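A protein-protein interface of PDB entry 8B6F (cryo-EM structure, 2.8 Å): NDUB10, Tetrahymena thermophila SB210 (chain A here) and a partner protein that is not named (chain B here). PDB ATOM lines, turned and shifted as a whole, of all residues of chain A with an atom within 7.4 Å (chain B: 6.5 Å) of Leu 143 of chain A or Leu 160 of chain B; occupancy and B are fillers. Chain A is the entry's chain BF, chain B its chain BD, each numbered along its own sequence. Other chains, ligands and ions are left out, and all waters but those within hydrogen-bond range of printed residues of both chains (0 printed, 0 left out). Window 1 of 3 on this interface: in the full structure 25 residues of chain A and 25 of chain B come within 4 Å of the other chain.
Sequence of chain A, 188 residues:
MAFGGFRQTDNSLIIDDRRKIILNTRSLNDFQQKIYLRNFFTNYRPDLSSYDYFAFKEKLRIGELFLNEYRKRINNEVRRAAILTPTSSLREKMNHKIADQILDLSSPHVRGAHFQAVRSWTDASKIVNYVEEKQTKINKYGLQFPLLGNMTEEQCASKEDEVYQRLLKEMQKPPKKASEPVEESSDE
Printed residues of chain B that touch a printed residue of chain A: Leu 160, Tyr 162, Ala 163, Pro 164, Ile 165 and Thr 166.
Hydrophobic or aromatic side chains of chain A within 4 Å of the printed part of chain B: Leu 143, Phe 145 and Pro 146.
Among the printed residues, 11 pairs touch across the chains.
Among the printed residues, no Asp or Glu carboxylate lies within 4 Å of a Lys or Arg side-chain nitrogen of the other chain.
Lys 137 of chain A touches none of the printed residues of chain B.
Printed residues of chain B within 4 Å of Gly 142 of chain A: Ile 165 (3.9 Å) and Thr 166 (2.9 Å).
Of chain B, only Leu 160 (3.5 Å), Ala 163 (3.7 Å) and Thr 166 (3.3 Å) come within 4 Å of Leu 143 of chain A.
Of the printed residues of chain B, Pro 146 of chain A touches Tyr 162 and Pro 164.
Printed residues of chain B within 4 Å of Lys 159 of chain A: Ile 165.
Gln 158 of chain B touches none of the printed residues of chain A.
Leu 160 of chain B touches just one residue of chain A: Leu 143 (3.5 Å).
Of the printed residues of chain A, Thr 166 of chain B touches Tyr 141, Gly 142 and Leu 143.
The nearest residue of chain A that does not touch Leu 160 of chain B is Tyr 141 of chain A (7.0 Å).
The nearest printed residue of chain A that does not touch Ile 165 of chain B is Val 163 of chain A (4.7 Å).
The backbone carbonyl oxygen (O) of Ile 138 of chain A sits at hydrogen-bond distance from the backbone NH (N) of Leu 143 of chain A (3.4 Å).
O of Asn 139 of chain A lies within hydrogen-bond range of NZ of Lys 159 of chain A (2.6 Å).
Among the printed residues, pairs that only touch across the chains: Pro 146 of chain A with Tyr 162 of chain B (2.8 Å), Leu 143 of chain A with Leu 160 of chain B (3.5 Å), Phe 145 of chain A with Ile 165 of chain B (3.5 Å), Leu 143 of chain A with Ala 163 of chain B (3.7 Å), Pro 146 of chain A with Pro 164 of chain B (3.7 Å), Phe 145 of chain A with Pro 164 of chain B (3.9 Å), Gly 142 of chain A with Ile 165 of chain B (3.9 Å) and Lys 159 of chain A with Ile 165 of chain B (3.9 Å).
The backbone carbonyl oxygen (O) of Tyr 141 of chain A sits at hydrogen-bond distance from the side-chain hydroxyl (OG1) of Thr 166 of chain B (2.4 Å).
The backbone carbonyl oxygen (O) of Gly 142 of chain A sits at hydrogen-bond distance from the side-chain hydroxyl (OG1) of Thr 166 of chain B (2.9 Å).
The backbone NH (N) of Leu 143 of chain A is in hydrogen-bond range of the side-chain hydroxyl (OG1) of Thr 166 of chain B (3.3 Å).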
ATOM      1  N   LYS A 137       0.984  -2.961  30.497  1.00  0.00           N
ATOM      2  CA  LYS A 137      -0.190  -3.575  31.105  1.00  0.00           C
ATOM      3  C   LYS A 137      -1.233  -3.920  30.050  1.00  0.00           C
ATOM      4  O   LYS A 137      -1.865  -4.980  30.112  1.00  0.00           O
ATOM      5  CB  LYS A 137      -0.773  -2.641  32.164  1.00  0.00           C
ATOM      6  CG  LYS A 137      -1.768  -3.311  33.094  1.00  0.00           C
ATOM      7  CD  LYS A 137      -2.153  -2.388  34.239  1.00  0.00           C
ATOM      8  CE  LYS A 137      -3.025  -3.107  35.254  1.00  0.00           C
ATOM      9  NZ  LYS A 137      -3.416  -2.215  36.384  1.00  0.00           N
ATOM     10  N   ILE A 138      -1.430  -3.034  29.074  1.00  0.00           N
ATOM     11  CA  ILE A 138      -2.389  -3.297  28.006  1.00  0.00           C
ATOM     12  C   ILE A 138      -1.923  -4.461  27.141  1.00  0.00           C
ATOM     13  O   ILE A 138      -2.697  -5.373  26.831  1.00  0.00           O
ATOM     14  CB  ILE A 138      -2.616  -2.020  27.174  1.00  0.00           C
ATOM     15  CG1 ILE A 138      -3.593  -1.094  27.897  1.00  0.00           C
ATOM     16  CG2 ILE A 138      -3.107  -2.349  25.765  1.00  0.00           C
ATOM     17  CD1 ILE A 138      -3.666   0.286  27.308  1.00  0.00           C
ATOM     18  N   ASN A 139      -0.652  -4.451  26.740  1.00  0.00           N
ATOM     19  CA  ASN A 139      -0.151  -5.473  25.830  1.00  0.00           C
ATOM     20  C   ASN A 139      -0.071  -6.849  26.479  1.00  0.00           C
ATOM     21  O   ASN A 139      -0.018  -7.853  25.761  1.00  0.00           O
ATOM     22  CB  ASN A 139       1.222  -5.071  25.296  1.00  0.00           C
ATOM     23  CG  ASN A 139       1.176  -3.791  24.487  1.00  0.00           C
ATOM     24  OD1 ASN A 139       0.212  -3.032  24.560  1.00  0.00           O
ATOM     25  ND2 ASN A 139       2.222  -3.547  23.707  1.00  0.00           N
ATOM     26  N   LYS A 140      -0.056  -6.924  27.812  1.00  0.00           N
ATOM     27  CA  LYS A 140      -0.127  -8.225  28.470  1.00  0.00           C
ATOM     28  C   LYS A 140      -1.344  -9.006  27.998  1.00  0.00           C
ATOM     29  O   LYS A 140      -1.251 -10.203  27.703  1.00  0.00           O
ATOM     30  CB  LYS A 140      -0.173  -8.056  29.990  1.00  0.00           C
ATOM     31  CG  LYS A 140       1.148  -7.656  30.620  1.00  0.00           C
ATOM     32  CD  LYS A 140       1.152  -7.898  32.122  1.00  0.00           C
ATOM     33  CE  LYS A 140      -0.028  -7.233  32.817  1.00  0.00           C
ATOM     34  NZ  LYS A 140       0.063  -7.354  34.300  1.00  0.00           N
ATOM     35  N   TYR A 141      -2.495  -8.344  27.923  1.00  0.00           N
ATOM     36  CA  TYR A 141      -3.734  -8.963  27.480  1.00  0.00           C
ATOM     37  C   TYR A 141      -4.078  -8.635  26.035  1.00  0.00           C
ATOM     38  O   TYR A 141      -5.117  -9.083  25.542  1.00  0.00           O
ATOM     39  CB  TYR A 141      -4.881  -8.535  28.399  1.00  0.00           C
ATOM     40  CG  TYR A 141      -4.537  -8.665  29.863  1.00  0.00           C
ATOM     41  CD1 TYR A 141      -4.477  -9.909  30.473  1.00  0.00           C
ATOM     42  CD2 TYR A 141      -4.267  -7.542  30.634  1.00  0.00           C
ATOM     43  CE1 TYR A 141      -4.157 -10.034  31.812  1.00  0.00           C
ATOM     44  CE2 TYR A 141      -3.947  -7.655  31.973  1.00  0.00           C
ATOM     45  CZ  TYR A 141      -3.894  -8.904  32.556  1.00  0.00           C
ATOM     46  OH  TYR A 141      -3.577  -9.024  33.888  1.00  0.00           O
ATOM     47  N   GLY A 142      -3.243  -7.864  25.348  1.00  0.00           N
ATOM     48  CA  GLY A 142      -3.453  -7.610  23.935  1.00  0.00           C
ATOM     49  C   GLY A 142      -4.708  -6.822  23.633  1.00  0.00           C
ATOM     50  O   GLY A 142      -5.447  -7.172  22.707  1.00  0.00           O
ATOM     51  N   LEU A 143      -4.965  -5.761  24.392  1.00  0.00           N
ATOM     52  CA  LEU A 143      -6.127  -4.913  24.182  1.00  0.00           C
ATOM     53  C   LEU A 143      -5.885  -3.836  23.135  1.00  0.00           C
ATOM     54  O   LEU A 143      -6.769  -3.003  22.913  1.00  0.00           O
ATOM     55  CB  LEU A 143      -6.544  -4.245  25.497  1.00  0.00           C
ATOM     56  CG  LEU A 143      -7.007  -5.146  26.640  1.00  0.00           C
ATOM     57  CD1 LEU A 143      -6.652  -4.527  27.975  1.00  0.00           C
ATOM     58  CD2 LEU A 143      -8.503  -5.379  26.540  1.00  0.00           C
ATOM     59  N   GLN A 144      -4.718  -3.828  22.491  1.00  0.00           N
ATOM     60  CA  GLN A 144      -4.326  -2.733  21.616  1.00  0.00           C
ATOM     61  C   GLN A 144      -4.363  -3.106  20.137  1.00  0.00           C
ATOM     62  O   GLN A 144      -3.759  -2.411  19.317  1.00  0.00           O
ATOM     63  CB  GLN A 144      -2.932  -2.235  22.003  1.00  0.00           C
ATOM     64  CG  GLN A 144      -1.759  -2.996  21.375  1.00  0.00           C
ATOM     65  CD  GLN A 144      -1.851  -4.499  21.558  1.00  0.00           C
ATOM     66  OE1 GLN A 144      -2.642  -4.994  22.357  1.00  0.00           O
ATOM     67  NE2 GLN A 144      -1.032  -5.234  20.817  1.00  0.00           N
ATOM     68  N   PHE A 145      -5.066  -4.180  19.768  1.00  0.00           N
ATOM     69  CA  PHE A 145      -5.047  -4.605  18.369  1.00  0.00           C
ATOM     70  C   PHE A 145      -5.686  -3.560  17.469  1.00  0.00           C
ATOM     71  O   PHE A 145      -4.988  -2.991  16.612  1.00  0.00           O
ATOM     72  CB  PHE A 145      -5.729  -5.964  18.211  1.00  0.00           C
ATOM     73  CG  PHE A 145      -6.285  -6.196  16.832  1.00  0.00           C
ATOM     74  CD1 PHE A 145      -5.470  -6.075  15.717  1.00  0.00           C
ATOM     75  CD2 PHE A 145      -7.611  -6.546  16.648  1.00  0.00           C
ATOM     76  CE1 PHE A 145      -5.970  -6.286  14.450  1.00  0.00           C
ATOM     77  CE2 PHE A 145      -8.119  -6.758  15.381  1.00  0.00           C
ATOM     78  CZ  PHE A 145      -7.297  -6.627  14.281  1.00  0.00           C
ATOM     79  N   PRO A 146      -6.983  -3.265  17.589  1.00  0.00           N
ATOM     80  CA  PRO A 146      -7.572  -2.263  16.694  1.00  0.00           C
ATOM     81  C   PRO A 146      -7.157  -0.851  17.055  1.00  0.00           C
ATOM     82  O   PRO A 146      -6.841  -0.055  16.163  1.00  0.00           O
ATOM     83  CB  PRO A 146      -9.077  -2.490  16.872  1.00  0.00           C
ATOM     84  CG  PRO A 146      -9.200  -2.950  18.277  1.00  0.00           C
ATOM     85  CD  PRO A 146      -7.949  -3.733  18.598  1.00  0.00           C
ATOM     86  N   LEU A 147      -7.141  -0.524  18.342  1.00  0.00           N
ATOM     87  CA  LEU A 147      -6.740   0.789  18.821  1.00  0.00           C
ATOM     88  C   LEU A 147      -5.327   0.712  19.381  1.00  0.00           C
ATOM     89  O   LEU A 147      -4.955  -0.275  20.019  1.00  0.00           O
ATOM     90  CB  LEU A 147      -7.695   1.289  19.907  1.00  0.00           C
ATOM     91  CG  LEU A 147      -9.085   1.779  19.490  1.00  0.00           C
ATOM     92  CD1 LEU A 147      -9.862   0.723  18.726  1.00  0.00           C
ATOM     93  CD2 LEU A 147      -9.867   2.215  20.716  1.00  0.00           C
ATOM     94  N   LEU A 148      -4.545   1.760  19.140  1.00  0.00           N
ATOM     95  CA  LEU A 148      -3.175   1.841  19.645  1.00  0.00           C
ATOM     96  C   LEU A 148      -2.335   0.660  19.168  1.00  0.00           C
ATOM     97  O   LEU A 148      -1.535   0.102  19.922  1.00  0.00           O
ATOM     98  CB  LEU A 148      -3.154   1.928  21.172  1.00  0.00           C
ATOM     99  CG  LEU A 148      -3.917   3.096  21.800  1.00  0.00           C
ATOM    100  CD1 LEU A 148      -3.850   3.007  23.310  1.00  0.00           C
ATOM    101  CD2 LEU A 148      -3.372   4.433  21.317  1.00  0.00           C
ATOM    102  N   GLY A 149      -2.509   0.273  17.907  1.00  0.00           N
ATOM    103  CA  GLY A 149      -1.716  -0.807  17.355  1.00  0.00           C
ATOM    104  C   GLY A 149      -2.239  -1.367  16.049  1.00  0.00           C
ATOM    105  O   GLY A 149      -3.429  -1.259  15.746  1.00  0.00           O
ATOM    106  N   LYS A 159      -1.185 -13.709  19.218  1.00  0.00           N
ATOM    107  CA  LYS A 159      -1.450 -12.924  20.418  1.00  0.00           C
ATOM    108  C   LYS A 159      -2.648 -13.470  21.184  1.00  0.00           C
ATOM    109  O   LYS A 159      -2.631 -13.513  22.418  1.00  0.00           O
ATOM    110  CB  LYS A 159      -1.675 -11.458  20.044  1.00  0.00           C
ATOM    111  CG  LYS A 159      -1.727 -10.505  21.234  1.00  0.00           C
ATOM    112  CD  LYS A 159      -0.387 -10.429  21.951  1.00  0.00           C
ATOM    113  CE  LYS A 159      -0.419  -9.425  23.089  1.00  0.00           C
ATOM    114  NZ  LYS A 159       0.886  -9.362  23.804  1.00  0.00           N
ATOM    115  N   VAL A 163      -2.422 -14.669  25.001  1.00  0.00           N
ATOM    116  CA  VAL A 163      -3.261 -14.080  26.041  1.00  0.00           C
ATOM    117  C   VAL A 163      -4.096 -15.155  26.721  1.00  0.00           C
ATOM    118  O   VAL A 163      -4.316 -15.114  27.936  1.00  0.00           O
ATOM    119  CB  VAL A 163      -4.140 -12.965  25.446  1.00  0.00           C
ATOM    120  CG1 VAL A 163      -5.141 -12.455  26.474  1.00  0.00           C
ATOM    121  CG2 VAL A 163      -3.270 -11.822  24.956  1.00  0.00           C
ATOM    122  N   LEU B 146     -17.341   4.873  23.280  1.00  0.00           N
ATOM    123  CA  LEU B 146     -17.089   4.526  24.678  1.00  0.00           C
ATOM    124  C   LEU B 146     -16.923   5.773  25.540  1.00  0.00           C
ATOM    125  O   LEU B 146     -15.933   5.934  26.252  1.00  0.00           O
ATOM    126  CB  LEU B 146     -15.859   3.633  24.780  1.00  0.00           C
ATOM    127  CG  LEU B 146     -15.965   2.218  24.210  1.00  0.00           C
ATOM    128  CD1 LEU B 146     -14.626   1.509  24.340  1.00  0.00           C
ATOM    129  CD2 LEU B 146     -17.062   1.420  24.899  1.00  0.00           C
ATOM    130  N   THR B 155     -19.588  -1.457  30.448  1.00  0.00           N
ATOM    131  CA  THR B 155     -19.200  -2.698  31.097  1.00  0.00           C
ATOM    132  C   THR B 155     -17.950  -3.274  30.441  1.00  0.00           C
ATOM    133  O   THR B 155     -17.454  -2.773  29.431  1.00  0.00           O
ATOM    134  CB  THR B 155     -20.343  -3.713  31.046  1.00  0.00           C
ATOM    135  OG1 THR B 155     -20.708  -3.964  29.683  1.00  0.00           O
ATOM    136  CG2 THR B 155     -21.551  -3.194  31.806  1.00  0.00           C
ATOM    137  N   LEU B 156     -17.430  -4.343  31.045  1.00  0.00           N
ATOM    138  CA  LEU B 156     -16.244  -4.992  30.498  1.00  0.00           C
ATOM    139  C   LEU B 156     -16.517  -5.548  29.107  1.00  0.00           C
ATOM    140  O   LEU B 156     -15.663  -5.460  28.218  1.00  0.00           O
ATOM    141  CB  LEU B 156     -15.768  -6.102  31.434  1.00  0.00           C
ATOM    142  CG  LEU B 156     -14.534  -6.875  30.965  1.00  0.00           C
ATOM    143  CD1 LEU B 156     -13.354  -5.943  30.749  1.00  0.00           C
ATOM    144  CD2 LEU B 156     -14.180  -7.964  31.959  1.00  0.00           C
ATOM    145  N   GLU B 157     -17.704  -6.120  28.897  1.00  0.00           N
ATOM    146  CA  GLU B 157     -18.042  -6.637  27.575  1.00  0.00           C
ATOM    147  C   GLU B 157     -18.095  -5.517  26.546  1.00  0.00           C
ATOM    148  O   GLU B 157     -17.588  -5.666  25.430  1.00  0.00           O
ATOM    149  CB  GLU B 157     -19.377  -7.380  27.622  1.00  0.00           C
ATOM    150  CG  GLU B 157     -19.313  -8.741  28.301  1.00  0.00           C
ATOM    151  CD  GLU B 157     -19.006  -8.646  29.782  1.00  0.00           C
ATOM    152  OE1 GLU B 157     -19.080  -7.528  30.335  1.00  0.00           O
ATOM    153  OE2 GLU B 157     -18.686  -9.687  30.394  1.00  0.00           O
ATOM    154  N   GLN B 158     -18.704  -4.384  26.901  1.00  0.00           N
ATOM    155  CA  GLN B 158     -18.764  -3.263  25.969  1.00  0.00           C
ATOM    156  C   GLN B 158     -17.368  -2.753  25.635  1.00  0.00           C
ATOM    157  O   GLN B 158     -17.070  -2.445  24.476  1.00  0.00           O
ATOM    158  CB  GLN B 158     -19.621  -2.142  26.553  1.00  0.00           C
ATOM    159  CG  GLN B 158     -21.078  -2.521  26.729  1.00  0.00           C
ATOM    160  CD  GLN B 158     -21.913  -1.378  27.261  1.00  0.00           C
ATOM    161  OE1 GLN B 158     -21.392  -0.316  27.594  1.00  0.00           O
ATOM    162  NE2 GLN B 158     -23.221  -1.587  27.339  1.00  0.00           N
ATOM    163  N   LYS B 159     -16.496  -2.652  26.640  1.00  0.00           N
ATOM    164  CA  LYS B 159     -15.134  -2.194  26.391  1.00  0.00           C
ATOM    165  C   LYS B 159     -14.357  -3.206  25.556  1.00  0.00           C
ATOM    166  O   LYS B 159     -13.548  -2.824  24.703  1.00  0.00           O
ATOM    167  CB  LYS B 159     -14.420  -1.914  27.712  1.00  0.00           C
ATOM    168  CG  LYS B 159     -14.721  -0.531  28.273  1.00  0.00           C
ATOM    169  CD  LYS B 159     -14.135  -0.330  29.659  1.00  0.00           C
ATOM    170  CE  LYS B 159     -14.942  -1.065  30.712  1.00  0.00           C
ATOM    171  NZ  LYS B 159     -14.476  -0.750  32.091  1.00  0.00           N
ATOM    172  N   LEU B 160     -14.585  -4.500  25.788  1.00  0.00           N
ATOM    173  CA  LEU B 160     -13.893  -5.527  25.019  1.00  0.00           C
ATOM    174  C   LEU B 160     -14.422  -5.645  23.597  1.00  0.00           C
ATOM    175  O   LEU B 160     -13.746  -6.237  22.749  1.00  0.00           O
ATOM    176  CB  LEU B 160     -13.999  -6.882  25.720  1.00  0.00           C
ATOM    177  CG  LEU B 160     -13.147  -7.087  26.975  1.00  0.00           C
ATOM    178  CD1 LEU B 160     -13.401  -8.462  27.563  1.00  0.00           C
ATOM    179  CD2 LEU B 160     -11.668  -6.909  26.678  1.00  0.00           C
ATOM    180  N   GLU B 161     -15.607  -5.106  23.311  1.00  0.00           N
ATOM    181  CA  GLU B 161     -16.094  -5.109  21.937  1.00  0.00           C
ATOM    182  C   GLU B 161     -15.140  -4.386  20.998  1.00  0.00           C
ATOM    183  O   GLU B 161     -15.189  -4.617  19.785  1.00  0.00           O
ATOM    184  CB  GLU B 161     -17.481  -4.468  21.864  1.00  0.00           C
ATOM    185  CG  GLU B 161     -18.607  -5.394  22.290  1.00  0.00           C
ATOM    186  CD  GLU B 161     -18.740  -6.608  21.390  1.00  0.00           C
ATOM    187  OE1 GLU B 161     -18.158  -6.598  20.286  1.00  0.00           O
ATOM    188  OE2 GLU B 161     -19.419  -7.575  21.791  1.00  0.00           O
ATOM    189  N   TYR B 162     -14.283  -3.516  21.524  1.00  0.00           N
ATOM    190  CA  TYR B 162     -13.224  -2.884  20.750  1.00  0.00           C
ATOM    191  C   TYR B 162     -11.871  -3.550  20.960  1.00  0.00           C
ATOM    192  O   TYR B 162     -10.846  -2.978  20.582  1.00  0.00           O
ATOM    193  CB  TYR B 162     -13.132  -1.398  21.103  1.00  0.00           C
ATOM    194  CG  TYR B 162     -14.347  -0.600  20.695  1.00  0.00           C
ATOM    195  CD1 TYR B 162     -15.470  -0.541  21.509  1.00  0.00           C
ATOM    196  CD2 TYR B 162     -14.369   0.101  19.497  1.00  0.00           C
ATOM    197  CE1 TYR B 162     -16.581   0.190  21.141  1.00  0.00           C
ATOM    198  CE2 TYR B 162     -15.476   0.836  19.119  1.00  0.00           C
ATOM    199  CZ  TYR B 162     -16.579   0.876  19.945  1.00  0.00           C
ATOM    200  OH  TYR B 162     -17.683   1.604  19.577  1.00  0.00           O
ATOM    201  N   ALA B 163     -11.843  -4.733  21.571  1.00  0.00           N
ATOM    202  CA  ALA B 163     -10.612  -5.495  21.788  1.00  0.00           C
ATOM    203  C   ALA B 163     -10.856  -6.938  21.367  1.00  0.00           C
ATOM    204  O   ALA B 163     -10.990  -7.832  22.211  1.00  0.00           O
ATOM    205  CB  ALA B 163     -10.164  -5.416  23.246  1.00  0.00           C
ATOM    206  N   PRO B 164     -10.927  -7.199  20.060  1.00  0.00           N
ATOM    207  CA  PRO B 164     -11.305  -8.550  19.610  1.00  0.00           C
ATOM    208  C   PRO B 164     -10.404  -9.651  20.138  1.00  0.00           C
ATOM    209  O   PRO B 164     -10.900 -10.728  20.486  1.00  0.00           O
ATOM    210  CB  PRO B 164     -11.230  -8.437  18.081  1.00  0.00           C
ATOM    211  CG  PRO B 164     -11.390  -6.992  17.795  1.00  0.00           C
ATOM    212  CD  PRO B 164     -10.731  -6.278  18.929  1.00  0.00           C
ATOM    213  N   ILE B 165      -9.091  -9.424  20.203  1.00  0.00           N
ATOM    214  CA  ILE B 165      -8.191 -10.472  20.677  1.00  0.00           C
ATOM    215  C   ILE B 165      -8.460 -10.778  22.144  1.00  0.00           C
ATOM    216  O   ILE B 165      -8.651 -11.937  22.529  1.00  0.00           O
ATOM    217  CB  ILE B 165      -6.722 -10.072  20.447  1.00  0.00           C
ATOM    218  CG1 ILE B 165      -6.460  -9.865  18.955  1.00  0.00           C
ATOM    219  CG2 ILE B 165      -5.786 -11.133  21.019  1.00  0.00           C
ATOM    220  CD1 ILE B 165      -5.058  -9.405  18.634  1.00  0.00           C
ATOM    221  N   THR B 166      -8.484  -9.744  22.984  1.00  0.00           N
ATOM    222  CA  THR B 166      -8.704  -9.964  24.408  1.00  0.00           C
ATOM    223  C   THR B 166     -10.097 -10.522  24.665  1.00  0.00           C
ATOM    224  O   THR B 166     -10.288 -11.337  25.573  1.00  0.00           O
ATOM    225  CB  THR B 166      -8.496  -8.664  25.178  1.00  0.00           C
ATOM    226  OG1 THR B 166      -7.224  -8.106  24.832  1.00  0.00           O
ATOM    227  CG2 THR B 166      -8.536  -8.923  26.674  1.00  0.00           C
ATOM    228  N   ARG B 167     -11.082 -10.086  23.879  1.00  0.00           N
ATOM    229  CA  ARG B 167     -12.438 -10.595  24.043  1.00  0.00           C
ATOM    230  C   ARG B 167     -12.477 -12.104  23.845  1.00  0.00           C
ATOM    231  O   ARG B 167     -12.997 -12.841  24.690  1.00  0.00           O
ATOM    232  CB  ARG B 167     -13.366  -9.893  23.053  1.00  0.00           C
ATOM    233  CG  ARG B 167     -14.805 -10.378  23.065  1.00  0.00           C
ATOM    234  CD  ARG B 167     -15.607  -9.657  21.998  1.00  0.00           C
ATOM    235  NE  ARG B 167     -15.033  -9.866  20.674  1.00  0.00           N
ATOM    236  CZ  ARG B 167     -15.285  -9.110  19.615  1.00  0.00           C
ATOM    237  NH1 ARG B 167     -16.096  -8.069  19.684  1.00  0.00           N
ATOM    238  NH2 ARG B 167     -14.702  -9.404  18.456  1.00  0.00           N
ATOM    239  N   TRP B 170     -10.414 -13.951  26.553  1.00  0.00           N
ATOM    240  CA  TRP B 170     -11.108 -13.944  27.838  1.00  0.00           C
ATOM    241  C   TRP B 170     -12.293 -14.901  27.834  1.00  0.00           C
ATOM    242  O   TRP B 170     -12.546 -15.584  28.833  1.00  0.00           O
ATOM    243  CB  TRP B 170     -11.553 -12.518  28.166  1.00  0.00           C
ATOM    244  CG  TRP B 170     -12.281 -12.375  29.464  1.00  0.00           C
ATOM    245  CD1 TRP B 170     -13.597 -12.063  29.630  1.00  0.00           C
ATOM    246  CD2 TRP B 170     -11.737 -12.534  30.780  1.00  0.00           C
ATOM    247  NE1 TRP B 170     -13.906 -12.018  30.966  1.00  0.00           N
ATOM    248  CE2 TRP B 170     -12.781 -12.303  31.693  1.00  0.00           C
ATOM    249  CE3 TRP B 170     -10.467 -12.848  31.273  1.00  0.00           C
ATOM    250  CZ2 TRP B 170     -12.596 -12.377  33.072  1.00  0.00           C
ATOM    251  CZ3 TRP B 170     -10.284 -12.921  32.642  1.00  0.00           C
ATOM    252  CH2 TRP B 170     -11.344 -12.687  33.526  1.00  0.00           C
